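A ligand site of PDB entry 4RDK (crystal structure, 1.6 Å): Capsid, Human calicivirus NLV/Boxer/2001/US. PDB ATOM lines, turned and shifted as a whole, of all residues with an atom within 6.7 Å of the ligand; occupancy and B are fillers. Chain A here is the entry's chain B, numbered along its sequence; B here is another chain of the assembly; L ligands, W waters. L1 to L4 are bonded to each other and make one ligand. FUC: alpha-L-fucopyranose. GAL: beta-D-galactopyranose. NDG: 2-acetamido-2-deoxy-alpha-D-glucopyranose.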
ATOM      1  N   ASP A 114       3.460   5.753   9.947  1.00  0.00           N
ATOM      2  CA  ASP A 114       3.933   6.615  11.025  1.00  0.00           C
ATOM      3  C   ASP A 114       5.024   5.884  11.797  1.00  0.00           C
ATOM      4  O   ASP A 114       4.769   4.837  12.415  1.00  0.00           O
ATOM      5  CB  ASP A 114       2.793   7.004  11.964  1.00  0.00           C
ATOM      6  CG  ASP A 114       1.795   7.968  11.335  1.00  0.00           C
ATOM      7  OD1 ASP A 114       1.941   8.310  10.128  1.00  0.00           O
ATOM      8  OD2 ASP A 114       0.858   8.391  12.047  1.00  0.00           O
ATOM      9  N   HIS A 116       7.286   5.676  14.893  1.00  0.00           N
ATOM     10  CA  HIS A 116       7.381   6.202  16.255  1.00  0.00           C
ATOM     11  C   HIS A 116       8.791   5.958  16.776  1.00  0.00           C
ATOM     12  O   HIS A 116       9.165   4.813  17.078  1.00  0.00           O
ATOM     13  CB  HIS A 116       6.311   5.572  17.141  1.00  0.00           C
ATOM     14  CG  HIS A 116       4.910   5.811  16.650  1.00  0.00           C
ATOM     15  ND1 HIS A 116       4.117   6.838  17.113  1.00  0.00           N
ATOM     16  CD2 HIS A 116       4.180   5.171  15.708  1.00  0.00           C
ATOM     17  CE1 HIS A 116       2.954   6.809  16.495  1.00  0.00           C
ATOM     18  NE2 HIS A 116       2.970   5.811  15.624  1.00  0.00           N
ATOM     19  N   VAL A 137       7.370  11.364  16.330  1.00  0.00           N
ATOM     20  CA  VAL A 137       6.804  10.655  15.188  1.00  0.00           C
ATOM     21  C   VAL A 137       7.347  11.207  13.880  1.00  0.00           C
ATOM     22  O   VAL A 137       7.445  12.437  13.702  1.00  0.00           O
ATOM     23  CB  VAL A 137       5.267  10.753  15.170  1.00  0.00           C
ATOM     24  CG1 VAL A 137       4.702  10.019  13.960  1.00  0.00           C
ATOM     25  CG2 VAL A 137       4.692  10.193  16.473  1.00  0.00           C
ATOM     26  N   HIS A 139       6.603  10.830   9.740  1.00  0.00           N
ATOM     27  CA  HIS A 139       5.823  10.274   8.624  1.00  0.00           C
ATOM     28  C   HIS A 139       6.749   9.859   7.486  1.00  0.00           C
ATOM     29  O   HIS A 139       7.534  10.677   7.007  1.00  0.00           O
ATOM     30  CB  HIS A 139       4.876  11.317   8.061  1.00  0.00           C
ATOM     31  CG  HIS A 139       3.808  11.748   9.015  1.00  0.00           C
ATOM     32  ND1 HIS A 139       3.009  12.839   8.791  1.00  0.00           N
ATOM     33  CD2 HIS A 139       3.421  11.228  10.205  1.00  0.00           C
ATOM     34  CE1 HIS A 139       2.147  12.976   9.787  1.00  0.00           C
ATOM     35  NE2 HIS A 139       2.385  12.006  10.660  1.00  0.00           N
ATOM     36  N   TRP A 174       8.129   1.737  17.430  1.00  0.00           N
ATOM     37  CA  TRP A 174       6.950   1.059  16.884  1.00  0.00           C
ATOM     38  C   TRP A 174       6.433   1.797  15.660  1.00  0.00           C
ATOM     39  O   TRP A 174       6.895   2.904  15.351  1.00  0.00           O
ATOM     40  CB  TRP A 174       5.867   0.856  17.949  1.00  0.00           C
ATOM     41  CG  TRP A 174       5.211   2.106  18.510  1.00  0.00           C
ATOM     42  CD1 TRP A 174       5.758   3.009  19.380  1.00  0.00           C
ATOM     43  CD2 TRP A 174       3.871   2.549  18.263  1.00  0.00           C
ATOM     44  NE1 TRP A 174       4.848   3.998  19.681  1.00  0.00           N
ATOM     45  CE2 TRP A 174       3.682   3.733  19.007  1.00  0.00           C
ATOM     46  CE3 TRP A 174       2.810   2.054  17.497  1.00  0.00           C
ATOM     47  CZ2 TRP A 174       2.475   4.434  18.997  1.00  0.00           C
ATOM     48  CZ3 TRP A 174       1.611   2.760  17.485  1.00  0.00           C
ATOM     49  CH2 TRP A 174       1.451   3.937  18.235  1.00  0.00           C
ATOM     50  N   VAL A 175       5.493   1.166  14.972  1.00  0.00           N
ATOM     51  CA  VAL A 175       4.976   1.694  13.720  1.00  0.00           C
ATOM     52  C   VAL A 175       3.453   1.614  13.719  1.00  0.00           C
ATOM     53  O   VAL A 175       2.885   0.634  14.213  1.00  0.00           O
ATOM     54  CB  VAL A 175       5.509   0.880  12.510  1.00  0.00           C
ATOM     55  CG1 VAL A 175       4.931   1.394  11.208  1.00  0.00           C
ATOM     56  CG2 VAL A 175       7.045   0.920  12.463  1.00  0.00           C
ATOM     57  N   SER A 176       2.790   2.628  13.189  1.00  0.00           N
ATOM     58  CA  SER A 176       1.346   2.568  13.001  1.00  0.00           C
ATOM     59  C   SER A 176       0.974   2.993  11.586  1.00  0.00           C
ATOM     60  O   SER A 176       1.801   3.551  10.856  1.00  0.00           O
ATOM     61  CB  SER A 176       0.625   3.441  14.039  1.00  0.00           C
ATOM     62  OG  SER A 176       1.009   4.808  13.927  1.00  0.00           O
ATOM     63  N   ASN A 177      -0.265   2.714  11.199  1.00  0.00           N
ATOM     64  CA  ASN A 177      -0.718   3.103   9.861  1.00  0.00           C
ATOM     65  C   ASN A 177      -0.929   4.605   9.761  1.00  0.00           C
ATOM     66  O   ASN A 177      -1.241   5.266  10.752  1.00  0.00           O
ATOM     67  CB  ASN A 177      -2.019   2.380   9.500  1.00  0.00           C
ATOM     68  CG  ASN A 177      -3.190   2.795  10.370  1.00  0.00           C
ATOM     69  OD1 ASN A 177      -3.263   2.415  11.540  1.00  0.00           O
ATOM     70  ND2 ASN A 177      -4.115   3.560   9.803  1.00  0.00           N
ATOM     71  N   ARG A 178      -0.720   5.123   8.566  1.00  0.00           N
ATOM     72  CA  ARG A 178      -1.102   6.483   8.211  1.00  0.00           C
ATOM     73  C   ARG A 178      -2.632   6.573   8.203  1.00  0.00           C
ATOM     74  O   ARG A 178      -3.305   5.664   7.729  1.00  0.00           O
ATOM     75  CB  ARG A 178      -0.561   6.788   6.818  1.00  0.00           C
ATOM     76  CG  ARG A 178      -0.994   8.112   6.230  1.00  0.00           C
ATOM     77  CD  ARG A 178      -0.470   8.279   4.814  1.00  0.00           C
ATOM     78  NE  ARG A 178      -0.925   9.545   4.246  1.00  0.00           N
ATOM     79  CZ  ARG A 178      -0.550  10.034   3.081  1.00  0.00           C
ATOM     80  NH1 ARG A 178       0.302   9.373   2.305  1.00  0.00           N
ATOM     81  NH2 ARG A 178      -1.042  11.200   2.671  1.00  0.00           N
ATOM     82  N   THR A 179      -3.187   7.663   8.736  1.00  0.00           N
ATOM     83  CA  THR A 179      -4.633   7.838   8.695  1.00  0.00           C
ATOM     84  C   THR A 179      -5.124   7.655   7.253  1.00  0.00           C
ATOM     85  O   THR A 179      -4.558   8.229   6.335  1.00  0.00           O
ATOM     86  CB  THR A 179      -5.051   9.228   9.207  1.00  0.00           C
ATOM     87  OG1 THR A 179      -4.528   9.416  10.533  1.00  0.00           O
ATOM     88  CG2 THR A 179      -6.573   9.360   9.243  1.00  0.00           C
ATOM     89  N   GLY A 180      -6.155   6.840   7.075  1.00  0.00           N
ATOM     90  CA  GLY A 180      -6.726   6.613   5.750  1.00  0.00           C
ATOM     91  C   GLY A 180      -6.107   5.464   4.960  1.00  0.00           C
ATOM     92  O   GLY A 180      -6.588   5.132   3.877  1.00  0.00           O
ATOM     93  N   ALA A 181      -5.072   4.845   5.505  1.00  0.00           N
ATOM     94  CA  ALA A 181      -4.380   3.765   4.809  1.00  0.00           C
ATOM     95  C   ALA A 181      -4.180   2.564   5.702  1.00  0.00           C
ATOM     96  O   ALA A 181      -4.217   2.684   6.924  1.00  0.00           O
ATOM     97  CB  ALA A 181      -3.039   4.261   4.273  1.00  0.00           C
ATOM     98  N   VAL A 224       1.900  -2.088  14.459  1.00  0.00           N
ATOM     99  CA  VAL A 224       0.551  -2.251  14.990  1.00  0.00           C
ATOM    100  C   VAL A 224      -0.471  -2.382  13.863  1.00  0.00           C
ATOM    101  O   VAL A 224      -0.484  -1.594  12.926  1.00  0.00           O
ATOM    102  CB  VAL A 224       0.187  -1.098  15.935  1.00  0.00           C
ATOM    103  CG1 VAL A 224      -1.255  -1.236  16.437  1.00  0.00           C
ATOM    104  CG2 VAL A 224       1.178  -1.078  17.109  1.00  0.00           C
ATOM    105  N   SER A 225      -1.319  -3.419  13.988  1.00  0.00           N
ATOM    106  CA  SER A 225      -2.313  -3.809  12.997  1.00  0.00           C
ATOM    107  C   SER A 225      -1.749  -4.821  11.997  1.00  0.00           C
ATOM    108  O   SER A 225      -2.485  -5.369  11.168  1.00  0.00           O
ATOM    109  CB  SER A 225      -2.928  -2.608  12.267  1.00  0.00           C
ATOM    110  OG  SER A 225      -2.172  -2.240  11.120  1.00  0.00           O
ATOM    111  N   LEU B 127      -1.211  -6.099  19.761  1.00  0.00           N
ATOM    112  CA  LEU B 127      -0.620  -5.221  18.756  1.00  0.00           C
ATOM    113  C   LEU B 127      -1.549  -4.995  17.557  1.00  0.00           C
ATOM    114  O   LEU B 127      -1.100  -4.798  16.433  1.00  0.00           O
ATOM    115  CB  LEU B 127       0.720  -5.795  18.296  1.00  0.00           C
ATOM    116  CG  LEU B 127       1.803  -5.861  19.384  1.00  0.00           C
ATOM    117  CD1 LEU B 127       3.029  -6.632  18.900  1.00  0.00           C
ATOM    118  CD2 LEU B 127       2.174  -4.456  19.818  1.00  0.00           C
ATOM    119  N   SER B 128      -2.856  -5.035  17.794  1.00  0.00           N
ATOM    120  CA  SER B 128      -3.804  -4.794  16.718  1.00  0.00           C
ATOM    121  C   SER B 128      -4.182  -3.311  16.613  1.00  0.00           C
ATOM    122  O   SER B 128      -4.520  -2.824  15.533  1.00  0.00           O
ATOM    123  CB  SER B 128      -5.054  -5.663  16.863  1.00  0.00           C
ATOM    124  OG  SER B 128      -5.883  -5.204  17.911  1.00  0.00           O
ATOM    125  N   THR B 129      -4.096  -2.597  17.733  1.00  0.00           N
ATOM    126  CA  THR B 129      -4.509  -1.200  17.785  1.00  0.00           C
ATOM    127  C   THR B 129      -3.850  -0.516  18.966  1.00  0.00           C
ATOM    128  O   THR B 129      -3.379  -1.183  19.894  1.00  0.00           O
ATOM    129  CB  THR B 129      -6.053  -1.080  17.908  1.00  0.00           C
ATOM    130  OG1 THR B 129      -6.445   0.292  17.878  1.00  0.00           O
ATOM    131  CG2 THR B 129      -6.533  -1.723  19.206  1.00  0.00           C
ATOM    132  N   GLY B 130      -3.790   0.811  18.936  1.00  0.00           N
ATOM    133  CA  GLY B 130      -3.263   1.578  20.057  1.00  0.00           C
ATOM    134  C   GLY B 130      -1.750   1.665  20.140  1.00  0.00           C
ATOM    135  O   GLY B 130      -1.033   1.062  19.337  1.00  0.00           O
ATOM    136  N   ASP B 131      -1.272   2.423  21.116  1.00  0.00           N
ATOM    137  CA  ASP B 131       0.161   2.629  21.382  1.00  0.00           C
ATOM    138  C   ASP B 131       0.655   1.558  22.350  1.00  0.00           C
ATOM    139  O   ASP B 131       0.206   1.489  23.501  1.00  0.00           O
ATOM    140  CB  ASP B 131       0.349   4.022  21.976  1.00  0.00           C
ATOM    141  CG  ASP B 131       1.805   4.370  22.243  1.00  0.00           C
ATOM    142  OD1 ASP B 131       2.666   3.461  22.215  1.00  0.00           O
ATOM    143  OD2 ASP B 131       2.085   5.566  22.500  1.00  0.00           O
ATOM    144  N   PRO B 132       1.568   0.684  21.883  1.00  0.00           N
ATOM    145  CA  PRO B 132       2.014  -0.431  22.721  1.00  0.00           C
ATOM    146  C   PRO B 132       3.222  -0.090  23.584  1.00  0.00           C
ATOM    147  O   PRO B 132       3.751  -0.983  24.263  1.00  0.00           O
ATOM    148  CB  PRO B 132       2.432  -1.472  21.674  1.00  0.00           C
ATOM    149  CG  PRO B 132       3.011  -0.615  20.551  1.00  0.00           C
ATOM    150  CD  PRO B 132       2.138   0.634  20.524  1.00  0.00           C
HETATM  151  C1  FUC L   1      -0.604   7.186  17.810  1.00  0.00           C
HETATM  152  C2  FUC L   1       0.118   8.147  18.718  1.00  0.00           C
HETATM  153  C3  FUC L   1      -0.828   8.836  19.637  1.00  0.00           C
HETATM  154  C4  FUC L   1      -1.616   7.906  20.402  1.00  0.00           C
HETATM  155  C5  FUC L   1      -2.289   6.929  19.509  1.00  0.00           C
HETATM  156  C6  FUC L   1      -3.001   5.916  20.292  1.00  0.00           C
HETATM  157  O2  FUC L   1       0.790   9.089  17.939  1.00  0.00           O
HETATM  158  O3  FUC L   1      -0.104   9.738  20.500  1.00  0.00           O
HETATM  159  O4  FUC L   1      -0.789   7.208  21.362  1.00  0.00           O
HETATM  160  O5  FUC L   1      -1.325   6.261  18.575  1.00  0.00           O
HETATM  161  C1  GAL L   2      -3.471   7.279  15.833  1.00  0.00           C
HETATM  162  C2  GAL L   2      -1.966   7.139  15.861  1.00  0.00           C
HETATM  163  C3  GAL L   2      -1.368   7.610  14.644  1.00  0.00           C
HETATM  164  C4  GAL L   2      -1.950   6.982  13.425  1.00  0.00           C
HETATM  165  C5  GAL L   2      -3.468   7.115  13.431  1.00  0.00           C
HETATM  166  C6  GAL L   2      -4.112   6.428  12.258  1.00  0.00           C
HETATM  167  O2  GAL L   2      -1.464   7.915  17.004  1.00  0.00           O
HETATM  168  O3  GAL L   2       0.050   7.394  14.662  1.00  0.00           O
HETATM  169  O4  GAL L   2      -1.591   5.646  13.344  1.00  0.00           O
HETATM  170  O5  GAL L   2      -4.030   6.630  14.613  1.00  0.00           O
HETATM  171  O6  GAL L   2      -5.492   6.721  12.073  1.00  0.00           O
HETATM  172  C1  NDG L   3      -7.159   8.177  18.494  1.00  0.00           C
HETATM  173  C2  NDG L   3      -5.717   8.003  18.128  1.00  0.00           C
HETATM  174  C3  NDG L   3      -5.508   6.966  17.111  1.00  0.00           C
HETATM  175  C4  NDG L   3      -6.157   5.749  17.450  1.00  0.00           C
HETATM  176  C5  NDG L   3      -7.609   5.986  17.780  1.00  0.00           C
HETATM  177  C6  NDG L   3      -8.295   4.749  18.228  1.00  0.00           C
HETATM  178  C7  NDG L   3      -4.510  10.185  18.599  1.00  0.00           C
HETATM  179  C8  NDG L   3      -3.978  11.516  18.133  1.00  0.00           C
HETATM  180  O5  NDG L   3      -7.752   6.971  18.853  1.00  0.00           O
HETATM  181  O3  NDG L   3      -4.030   6.748  16.958  1.00  0.00           O
HETATM  182  O4  NDG L   3      -6.057   4.796  16.318  1.00  0.00           O
HETATM  183  O6  NDG L   3      -7.851   4.165  19.425  1.00  0.00           O
HETATM  184  O7  NDG L   3      -4.391   9.838  19.758  1.00  0.00           O
HETATM  185  N2  NDG L   3      -5.173   9.318  17.672  1.00  0.00           N
HETATM  186  O1  NDG L   3      -7.863   8.726  17.420  1.00  0.00           O
HETATM  187  C1  FUC L   4      -5.818   3.480  16.679  1.00  0.00           C
HETATM  188  C2  FUC L   4      -6.038   2.626  15.482  1.00  0.00           C
HETATM  189  C3  FUC L   4      -5.048   2.892  14.485  1.00  0.00           C
HETATM  190  C4  FUC L   4      -3.675   2.707  14.994  1.00  0.00           C
HETATM  191  C5  FUC L   4      -3.429   3.519  16.253  1.00  0.00           C
HETATM  192  C6  FUC L   4      -2.077   3.195  16.831  1.00  0.00           C
HETATM  193  O2  FUC L   4      -7.372   2.880  14.960  1.00  0.00           O
HETATM  194  O3  FUC L   4      -5.290   2.060  13.299  1.00  0.00           O
HETATM  195  O4  FUC L   4      -3.414   1.343  15.266  1.00  0.00           O
HETATM  196  O5  FUC L   4      -4.433   3.302  17.207  1.00  0.00           O
HETATM  197  O   HOH W   1      -6.928   5.771  21.586  1.00  0.00           O
HETATM  198  O   HOH W   2      -8.900   0.888  16.579  1.00  0.00           O
HETATM  199  O   HOH W   3      -6.839   1.622  20.405  1.00  0.00           O
HETATM  200  O   HOH W   4      -5.670  10.390  15.129  1.00  0.00           O
HETATM  201  O   HOH W   5       1.518   8.253  22.466  1.00  0.00           O
HETATM  202  O   HOH W   6      -2.053   6.210  23.546  1.00  0.00           O
HETATM  203  O   HOH W   7      -1.672   0.895  13.259  1.00  0.00           O
HETATM  204  O   HOH W   8      -6.634   4.473  11.051  1.00  0.00           O
HETATM  205  O   HOH W   9       2.706  10.597  19.436  1.00  0.00           O
HETATM  206  O   HOH W  10      -7.112   8.051  13.825  1.00  0.00           O
HETATM  207  O   HOH W  11      -5.546  -0.684  14.029  1.00  0.00           O
HETATM  208  O   HOH W  12      -5.753   8.220  21.759  1.00  0.00           O
HETATM  209  O   HOH W  13      -0.496  11.099  16.518  1.00  0.00           O
HETATM  210  O   HOH W  14      -7.741   5.508  14.191  1.00  0.00           O
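Merely in contact with the ligand: Thr 129 of chain B, Val 224 and Trp 174.
The side-chain carboxylate of Asp 131 of chain B lies close to an oxygen (O4) of FUC L1, at 3.5 Å.
The side-chain carboxylate (OD2) of Asp 114 sits at hydrogen-bond distance from an oxygen (O3) of GAL L2, at 2.9 Å.
O3 of GAL L2 sits at hydrogen-bond distance from NE2 of His 116, 3.5 Å away.
An oxygen (O4) of GAL L2 is in hydrogen-bond range of the backbone carbonyl oxygen of Asn 177.
OD1 of Asn 177 sits at hydrogen-bond distance from O3 of FUC L4 (2.7 Å).
The side-chain hydroxyl of Thr 179 lies within hydrogen-bond range of an oxygen (O6) of GAL L2 (3.3 Å).
The side-chain hydroxyl (OG) of Ser 176 is in hydrogen-bond range of an oxygen (O4) of GAL L2 (2.8 Å).
O5 of FUC L4 is in hydrogen-bond range of N of Gly 130 of chain B (3.1 Å).
Water W7 lies within hydrogen-bond range of an oxygen (O4) of FUC L4, the backbone carbonyl oxygen of Val 224 and the side-chain amide oxygen of Asn 177.
Water W8 lies within hydrogen-bond range of O6 of GAL L2 (2.7 Å) and ND2 of Asn 177 (3.0 Å).
Water W5 lies within hydrogen-bond range of the side-chain carboxylate (OD2) of Asp 131 of chain B (2.7 Å) and an oxygen (O4) of FUC L1 (2.8 Å).
Water W11 lies within hydrogen-bond range of the backbone carbonyl oxygen of Ser 128 of chain B and an oxygen (O3) of FUC L4.
Water W3 lies within hydrogen-bond range of OG1 of Thr 129 of chain B (2.9 Å), O6 of NDG L3 (2.9 Å) and N of Gly 130 of chain B (3.5 Å).
Water W2 lies within hydrogen-bond range of OG1 of Thr 129 of chain B and O2 of FUC L4.
The backbone NH (N) of His 116 sits at hydrogen-bond distance from the backbone carbonyl oxygen (O) of Trp 174, at 2.8 Å.
The backbone carbonyl oxygen (O) of Ala 181 lies within hydrogen-bond range of the side-chain amide nitrogen (ND2) of Asn 177 (3.0 Å).
NE2 of His 116 sits at hydrogen-bond distance from OG of Ser 176 (2.8 Å).
OD1 of Asp 131 of chain B sits close to NE1 of Trp 174, at 3.4 Å.
O of Val 175 is in hydrogen-bond range of N of Val 224, 2.9 Å away.
O of Ser 176 is in hydrogen-bond range of N of Asp 114 (2.9 Å).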
